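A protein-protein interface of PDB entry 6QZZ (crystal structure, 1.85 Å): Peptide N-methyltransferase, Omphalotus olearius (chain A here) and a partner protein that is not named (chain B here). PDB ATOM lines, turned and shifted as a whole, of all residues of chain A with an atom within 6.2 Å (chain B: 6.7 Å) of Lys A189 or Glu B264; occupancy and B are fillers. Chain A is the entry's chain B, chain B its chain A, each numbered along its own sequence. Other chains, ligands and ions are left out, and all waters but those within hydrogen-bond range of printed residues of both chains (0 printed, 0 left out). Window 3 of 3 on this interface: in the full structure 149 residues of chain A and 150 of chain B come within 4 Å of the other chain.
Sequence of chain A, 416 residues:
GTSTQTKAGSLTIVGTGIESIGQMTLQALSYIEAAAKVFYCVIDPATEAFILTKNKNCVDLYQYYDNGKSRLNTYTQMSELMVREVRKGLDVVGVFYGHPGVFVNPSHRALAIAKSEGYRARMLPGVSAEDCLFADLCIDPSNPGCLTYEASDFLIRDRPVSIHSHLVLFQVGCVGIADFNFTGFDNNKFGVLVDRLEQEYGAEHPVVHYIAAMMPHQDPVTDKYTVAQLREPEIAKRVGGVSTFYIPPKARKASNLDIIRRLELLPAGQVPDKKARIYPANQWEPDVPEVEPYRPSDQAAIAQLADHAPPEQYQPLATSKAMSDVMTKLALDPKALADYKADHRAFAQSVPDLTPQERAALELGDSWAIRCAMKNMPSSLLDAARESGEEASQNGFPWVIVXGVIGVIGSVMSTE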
ATOM      1  N   LEU A 155      23.350  29.373 -18.466  1.00  0.00           N
ATOM      2  CA  LEU A 155      22.152  29.081 -17.631  1.00  0.00           C
ATOM      3  C   LEU A 155      21.708  30.335 -16.877  1.00  0.00           C
ATOM      4  O   LEU A 155      20.518  30.706 -16.980  1.00  0.00           O
ATOM      5  CB  LEU A 155      22.486  27.943 -16.669  1.00  0.00           C
ATOM      6  CG  LEU A 155      22.718  26.601 -17.350  1.00  0.00           C
ATOM      7  CD1 LEU A 155      23.159  25.552 -16.352  1.00  0.00           C
ATOM      8  CD2 LEU A 155      21.469  26.156 -18.076  1.00  0.00           C
ATOM      9  N   VAL A 175      29.421  23.271 -13.409  1.00  0.00           N
ATOM     10  CA  VAL A 175      28.206  24.142 -13.441  1.00  0.00           C
ATOM     11  C   VAL A 175      27.927  24.682 -12.032  1.00  0.00           C
ATOM     12  O   VAL A 175      27.758  23.876 -11.088  1.00  0.00           O
ATOM     13  CB  VAL A 175      26.995  23.385 -14.027  1.00  0.00           C
ATOM     14  CG1 VAL A 175      25.708  24.184 -13.897  1.00  0.00           C
ATOM     15  CG2 VAL A 175      27.227  22.987 -15.471  1.00  0.00           C
ATOM     16  N   GLY A 176      27.912  26.010 -11.884  1.00  0.00           N
ATOM     17  CA  GLY A 176      27.556  26.692 -10.625  1.00  0.00           C
ATOM     18  C   GLY A 176      28.646  26.623  -9.567  1.00  0.00           C
ATOM     19  O   GLY A 176      28.373  27.031  -8.443  1.00  0.00           O
ATOM     20  N   ASP A 186      32.260  16.631  -7.898  1.00  0.00           N
ATOM     21  CA  ASP A 186      30.852  16.197  -8.090  1.00  0.00           C
ATOM     22  C   ASP A 186      30.098  17.364  -8.736  1.00  0.00           C
ATOM     23  O   ASP A 186      29.721  18.324  -8.016  1.00  0.00           O
ATOM     24  CB  ASP A 186      30.190  15.789  -6.766  1.00  0.00           C
ATOM     25  CG  ASP A 186      30.508  14.374  -6.307  1.00  0.00           C
ATOM     26  OD1 ASP A 186      30.869  13.543  -7.170  1.00  0.00           O
ATOM     27  OD2 ASP A 186      30.390  14.111  -5.089  1.00  0.00           O
ATOM     28  N   ASN A 187      29.946  17.287 -10.055  1.00  0.00           N
ATOM     29  CA  ASN A 187      29.224  18.246 -10.934  1.00  0.00           C
ATOM     30  C   ASN A 187      27.721  18.028 -10.716  1.00  0.00           C
ATOM     31  O   ASN A 187      27.050  17.572 -11.653  1.00  0.00           O
ATOM     32  CB  ASN A 187      29.692  18.021 -12.380  1.00  0.00           C
ATOM     33  CG  ASN A 187      29.205  19.028 -13.402  1.00  0.00           C
ATOM     34  OD1 ASN A 187      29.056  20.210 -13.117  1.00  0.00           O
ATOM     35  ND2 ASN A 187      29.002  18.568 -14.624  1.00  0.00           N
ATOM     36  N   ASN A 188      27.221  18.322  -9.509  1.00  0.00           N
ATOM     37  CA  ASN A 188      25.863  17.925  -9.042  1.00  0.00           C
ATOM     38  C   ASN A 188      24.774  18.749  -9.730  1.00  0.00           C
ATOM     39  O   ASN A 188      23.630  18.274  -9.728  1.00  0.00           O
ATOM     40  CB  ASN A 188      25.707  18.046  -7.523  1.00  0.00           C
ATOM     41  CG  ASN A 188      26.358  16.891  -6.797  1.00  0.00           C
ATOM     42  OD1 ASN A 188      26.252  15.744  -7.232  1.00  0.00           O
ATOM     43  ND2 ASN A 188      27.037  17.187  -5.701  1.00  0.00           N
ATOM     44  N   LYS A 189      25.100  19.925 -10.276  1.00  0.00           N
ATOM     45  CA  LYS A 189      24.105  20.803 -10.951  1.00  0.00           C
ATOM     46  C   LYS A 189      24.124  20.563 -12.468  1.00  0.00           C
ATOM     47  O   LYS A 189      23.485  21.363 -13.179  1.00  0.00           O
ATOM     48  CB  LYS A 189      24.368  22.269 -10.600  1.00  0.00           C
ATOM     49  CG  LYS A 189      24.287  22.593  -9.114  1.00  0.00           C
ATOM     50  CD  LYS A 189      22.965  22.181  -8.495  1.00  0.00           C
ATOM     51  CE  LYS A 189      22.776  22.689  -7.079  1.00  0.00           C
ATOM     52  NZ  LYS A 189      23.805  22.130  -6.174  1.00  0.00           N
ATOM     53  N   PHE A 190      24.777  19.490 -12.933  1.00  0.00           N
ATOM     54  CA  PHE A 190      24.877  19.113 -14.370  1.00  0.00           C
ATOM     55  C   PHE A 190      23.470  18.955 -14.950  1.00  0.00           C
ATOM     56  O   PHE A 190      23.250  19.362 -16.105  1.00  0.00           O
ATOM     57  CB  PHE A 190      25.680  17.824 -14.569  1.00  0.00           C
ATOM     58  CG  PHE A 190      25.788  17.359 -16.004  1.00  0.00           C
ATOM     59  CD1 PHE A 190      26.468  18.112 -16.952  1.00  0.00           C
ATOM     60  CD2 PHE A 190      25.219  16.161 -16.404  1.00  0.00           C
ATOM     61  CE1 PHE A 190      26.583  17.675 -18.263  1.00  0.00           C
ATOM     62  CE2 PHE A 190      25.330  15.730 -17.715  1.00  0.00           C
ATOM     63  CZ  PHE A 190      26.016  16.485 -18.641  1.00  0.00           C
ATOM     64  N   GLY A 191      22.549  18.390 -14.171  1.00  0.00           N
ATOM     65  CA  GLY A 191      21.162  18.118 -14.599  1.00  0.00           C
ATOM     66  C   GLY A 191      20.426  19.388 -14.991  1.00  0.00           C
ATOM     67  O   GLY A 191      19.514  19.298 -15.813  1.00  0.00           O
ATOM     68  N   VAL A 192      20.811  20.539 -14.427  1.00  0.00           N
ATOM     69  CA  VAL A 192      20.219  21.869 -14.767  1.00  0.00           C
ATOM     70  C   VAL A 192      20.600  22.226 -16.212  1.00  0.00           C
ATOM     71  O   VAL A 192      19.756  22.761 -16.941  1.00  0.00           O
ATOM     72  CB  VAL A 192      20.677  22.955 -13.774  1.00  0.00           C
ATOM     73  CG1 VAL A 192      20.116  24.322 -14.140  1.00  0.00           C
ATOM     74  CG2 VAL A 192      20.308  22.600 -12.337  1.00  0.00           C
ATOM     75  N   LEU A 193      21.838  21.953 -16.620  1.00  0.00           N
ATOM     76  CA  LEU A 193      22.286  22.228 -18.012  1.00  0.00           C
ATOM     77  C   LEU A 193      21.486  21.347 -18.981  1.00  0.00           C
ATOM     78  O   LEU A 193      20.967  21.884 -19.977  1.00  0.00           O
ATOM     79  CB  LEU A 193      23.789  21.963 -18.138  1.00  0.00           C
ATOM     80  CG  LEU A 193      24.337  22.010 -19.565  1.00  0.00           C
ATOM     81  CD1 LEU A 193      24.026  23.345 -20.226  1.00  0.00           C
ATOM     82  CD2 LEU A 193      25.829  21.721 -19.575  1.00  0.00           C
ATOM     83  N   VAL A 194      21.378  20.049 -18.690  1.00  0.00           N
ATOM     84  CA  VAL A 194      20.651  19.065 -19.546  1.00  0.00           C
ATOM     85  C   VAL A 194      19.196  19.523 -19.714  1.00  0.00           C
ATOM     86  O   VAL A 194      18.652  19.368 -20.832  1.00  0.00           O
ATOM     87  CB  VAL A 194      20.724  17.635 -18.977  1.00  0.00           C
ATOM     88  CG1 VAL A 194      20.033  16.636 -19.891  1.00  0.00           C
ATOM     89  CG2 VAL A 194      22.153  17.189 -18.696  1.00  0.00           C
ATOM     90  N   ILE B 259      17.285  29.638 -12.058  1.00  0.00           N
ATOM     91  CA  ILE B 259      18.642  29.018 -12.134  1.00  0.00           C
ATOM     92  C   ILE B 259      19.426  29.390 -10.868  1.00  0.00           C
ATOM     93  O   ILE B 259      20.114  28.506 -10.344  1.00  0.00           O
ATOM     94  CB  ILE B 259      19.381  29.417 -13.434  1.00  0.00           C
ATOM     95  CG1 ILE B 259      18.635  28.943 -14.690  1.00  0.00           C
ATOM     96  CG2 ILE B 259      20.816  28.922 -13.411  1.00  0.00           C
ATOM     97  CD1 ILE B 259      18.478  27.436 -14.829  1.00  0.00           C
ATOM     98  N   ILE B 260      19.334  30.644 -10.417  1.00  0.00           N
ATOM     99  CA  ILE B 260      19.885  31.115  -9.112  1.00  0.00           C
ATOM    100  C   ILE B 260      19.456  30.129  -8.015  1.00  0.00           C
ATOM    101  O   ILE B 260      20.329  29.735  -7.209  1.00  0.00           O
ATOM    102  CB  ILE B 260      19.435  32.559  -8.790  1.00  0.00           C
ATOM    103  CG1 ILE B 260      20.159  33.612  -9.632  1.00  0.00           C
ATOM    104  CG2 ILE B 260      19.551  32.854  -7.304  1.00  0.00           C
ATOM    105  CD1 ILE B 260      21.666  33.494  -9.641  1.00  0.00           C
ATOM    106  N   ARG B 261      18.180  29.732  -7.989  1.00  0.00           N
ATOM    107  CA  ARG B 261      17.643  28.781  -6.978  1.00  0.00           C
ATOM    108  C   ARG B 261      18.218  27.386  -7.214  1.00  0.00           C
ATOM    109  O   ARG B 261      18.695  26.774  -6.242  1.00  0.00           O
ATOM    110  CB  ARG B 261      16.119  28.713  -7.025  1.00  0.00           C
ATOM    111  CG  ARG B 261      15.457  29.901  -6.360  1.00  0.00           C
ATOM    112  CD  ARG B 261      13.962  29.752  -6.391  1.00  0.00           C
ATOM    113  NE  ARG B 261      13.399  30.887  -5.696  1.00  0.00           N
ATOM    114  CZ  ARG B 261      12.129  31.251  -5.729  1.00  0.00           C
ATOM    115  NH1 ARG B 261      11.755  32.311  -5.037  1.00  0.00           N
ATOM    116  NH2 ARG B 261      11.247  30.576  -6.450  1.00  0.00           N
ATOM    117  N   ARG B 262      18.194  26.904  -8.457  1.00  0.00           N
ATOM    118  CA  ARG B 262      18.596  25.509  -8.761  1.00  0.00           C
ATOM    119  C   ARG B 262      20.111  25.344  -8.584  1.00  0.00           C
ATOM    120  O   ARG B 262      20.523  24.210  -8.310  1.00  0.00           O
ATOM    121  CB  ARG B 262      18.109  25.119 -10.153  1.00  0.00           C
ATOM    122  CG  ARG B 262      16.591  25.138 -10.274  1.00  0.00           C
ATOM    123  CD  ARG B 262      16.148  24.603 -11.613  1.00  0.00           C
ATOM    124  NE  ARG B 262      16.452  23.181 -11.671  1.00  0.00           N
ATOM    125  CZ  ARG B 262      16.435  22.435 -12.769  1.00  0.00           C
ATOM    126  NH1 ARG B 262      16.734  21.149 -12.674  1.00  0.00           N
ATOM    127  NH2 ARG B 262      16.127  22.962 -13.947  1.00  0.00           N
ATOM    128  N   LEU B 263      20.897  26.421  -8.714  1.00  0.00           N
ATOM    129  CA  LEU B 263      22.377  26.402  -8.521  1.00  0.00           C
ATOM    130  C   LEU B 263      22.748  26.856  -7.101  1.00  0.00           C
ATOM    131  O   LEU B 263      23.950  26.996  -6.827  1.00  0.00           O
ATOM    132  CB  LEU B 263      23.059  27.305  -9.557  1.00  0.00           C
ATOM    133  CG  LEU B 263      22.889  26.941 -11.033  1.00  0.00           C
ATOM    134  CD1 LEU B 263      23.837  27.777 -11.878  1.00  0.00           C
ATOM    135  CD2 LEU B 263      23.113  25.457 -11.297  1.00  0.00           C
ATOM    136  N   GLU B 264      21.757  27.114  -6.250  1.00  0.00           N
ATOM    137  CA  GLU B 264      21.912  27.413  -4.799  1.00  0.00           C
ATOM    138  C   GLU B 264      22.861  28.602  -4.592  1.00  0.00           C
ATOM    139  O   GLU B 264      23.595  28.600  -3.591  1.00  0.00           O
ATOM    140  CB  GLU B 264      22.364  26.156  -4.051  1.00  0.00           C
ATOM    141  CG  GLU B 264      21.305  25.064  -4.035  1.00  0.00           C
ATOM    142  CD  GLU B 264      21.784  23.672  -3.662  1.00  0.00           C
ATOM    143  OE1 GLU B 264      20.945  22.758  -3.617  1.00  0.00           O
ATOM    144  OE2 GLU B 264      22.992  23.500  -3.433  1.00  0.00           O
ATOM    145  N   LEU B 265      22.815  29.601  -5.479  1.00  0.00           N
ATOM    146  CA  LEU B 265      23.480  30.918  -5.283  1.00  0.00           C
ATOM    147  C   LEU B 265      22.553  31.761  -4.400  1.00  0.00           C
ATOM    148  O   LEU B 265      22.409  32.975  -4.647  1.00  0.00           O
ATOM    149  CB  LEU B 265      23.741  31.548  -6.654  1.00  0.00           C
ATOM    150  CG  LEU B 265      24.532  30.670  -7.623  1.00  0.00           C
ATOM    151  CD1 LEU B 265      24.436  31.200  -9.048  1.00  0.00           C
ATOM    152  CD2 LEU B 265      25.990  30.564  -7.194  1.00  0.00           C
ATOM    153  N   LEU B 266      22.010  31.111  -3.364  1.00  0.00           N
ATOM    154  CA  LEU B 266      20.600  31.260  -2.907  1.00  0.00           C
ATOM    155  C   LEU B 266      20.363  32.641  -2.307  1.00  0.00           C
ATOM    156  O   LEU B 266      19.451  33.329  -2.763  1.00  0.00           O
ATOM    157  CB  LEU B 266      20.240  30.132  -1.930  1.00  0.00           C
ATOM    158  CG  LEU B 266      19.441  28.975  -2.536  1.00  0.00           C
ATOM    159  CD1 LEU B 266      19.508  27.735  -1.652  1.00  0.00           C
ATOM    160  CD2 LEU B 266      17.992  29.372  -2.790  1.00  0.00           C
ATOM    161  N   PRO B 267      21.143  33.098  -1.296  1.00  0.00           N
ATOM    162  CA  PRO B 267      20.903  34.409  -0.690  1.00  0.00           C
ATOM    163  C   PRO B 267      20.829  35.450  -1.820  1.00  0.00           C
ATOM    164  O   PRO B 267      21.861  35.946  -2.239  1.00  0.00           O
ATOM    165  CB  PRO B 267      22.086  34.612   0.270  1.00  0.00           C
ATOM    166  CG  PRO B 267      22.572  33.206   0.560  1.00  0.00           C
ATOM    167  CD  PRO B 267      22.310  32.420  -0.708  1.00  0.00           C
ATOM    168  N   ILE B 409      29.710  35.792  -5.058  1.00  0.00           N
ATOM    169  CA  ILE B 409      29.012  35.039  -3.966  1.00  0.00           C
ATOM    170  C   ILE B 409      30.051  34.205  -3.197  1.00  0.00           C
ATOM    171  O   ILE B 409      30.247  34.469  -1.988  1.00  0.00           O
ATOM    172  CB  ILE B 409      27.869  34.156  -4.515  1.00  0.00           C
ATOM    173  CG1 ILE B 409      26.789  34.968  -5.233  1.00  0.00           C
ATOM    174  CG2 ILE B 409      27.263  33.308  -3.409  1.00  0.00           C
ATOM    175  CD1 ILE B 409      26.248  36.102  -4.420  1.00  0.00           C
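The side-chain amino group (NZ) of Lys A189 lies within salt-bridge range of the side-chain carboxylate (OE2) of Glu B264 (3.2 Å).
The backbone NH (N) of Val A175 lies within hydrogen-bond range of the side-chain amide oxygen (OD1) of Asn A187 (3.1 Å).
Among the printed residues, merely in contact across the chains: Leu A155 with Ile B259, Val A175 with Leu B263, Lys A189 with Arg B262, Lys A189 with Leu B263, Val A192 with Ile B259 and Val A192 with Arg B262.
Printed residues of chain B within 4 Å of Leu A155: Ile B259. Of the printed residues of chain B, Val A175 touches Leu B263 (3.9 Å). Lys A189 touches three residues of chain B. Printed residues of chain B within 4 Å of Val A192: Ile B259 (3.6 Å) and Arg B262 (3.9 Å). Printed residues of chain A within 4 Å of Ile B259: Leu A155 (3.4 Å) and Val A192 (3.6 Å). Of the printed residues of chain A, Leu B263 touches Val A175 (3.9 Å) and Lys A189 (3.5 Å). Glu B264 touches just one residue of chain A: Lys A189. Leu B266 touches none of the printed residues of chain A. The nearest printed residue of chain A that does not touch Leu B263 is Gly A176 (4.1 Å).
Of the 10 printed residues of chain B, 4 touch a printed residue of chain A. Hydrophobic or aromatic side chains of chain B within 4 Å of the printed part of chain A: Ile B259 and Leu B263. Of the 12 printed residues of chain A, 4 touch a printed residue of chain B. Hydrophobic or aromatic side chains of chain A within 4 Å of the printed part of chain B: Leu A155, Val A175 and Val A192.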
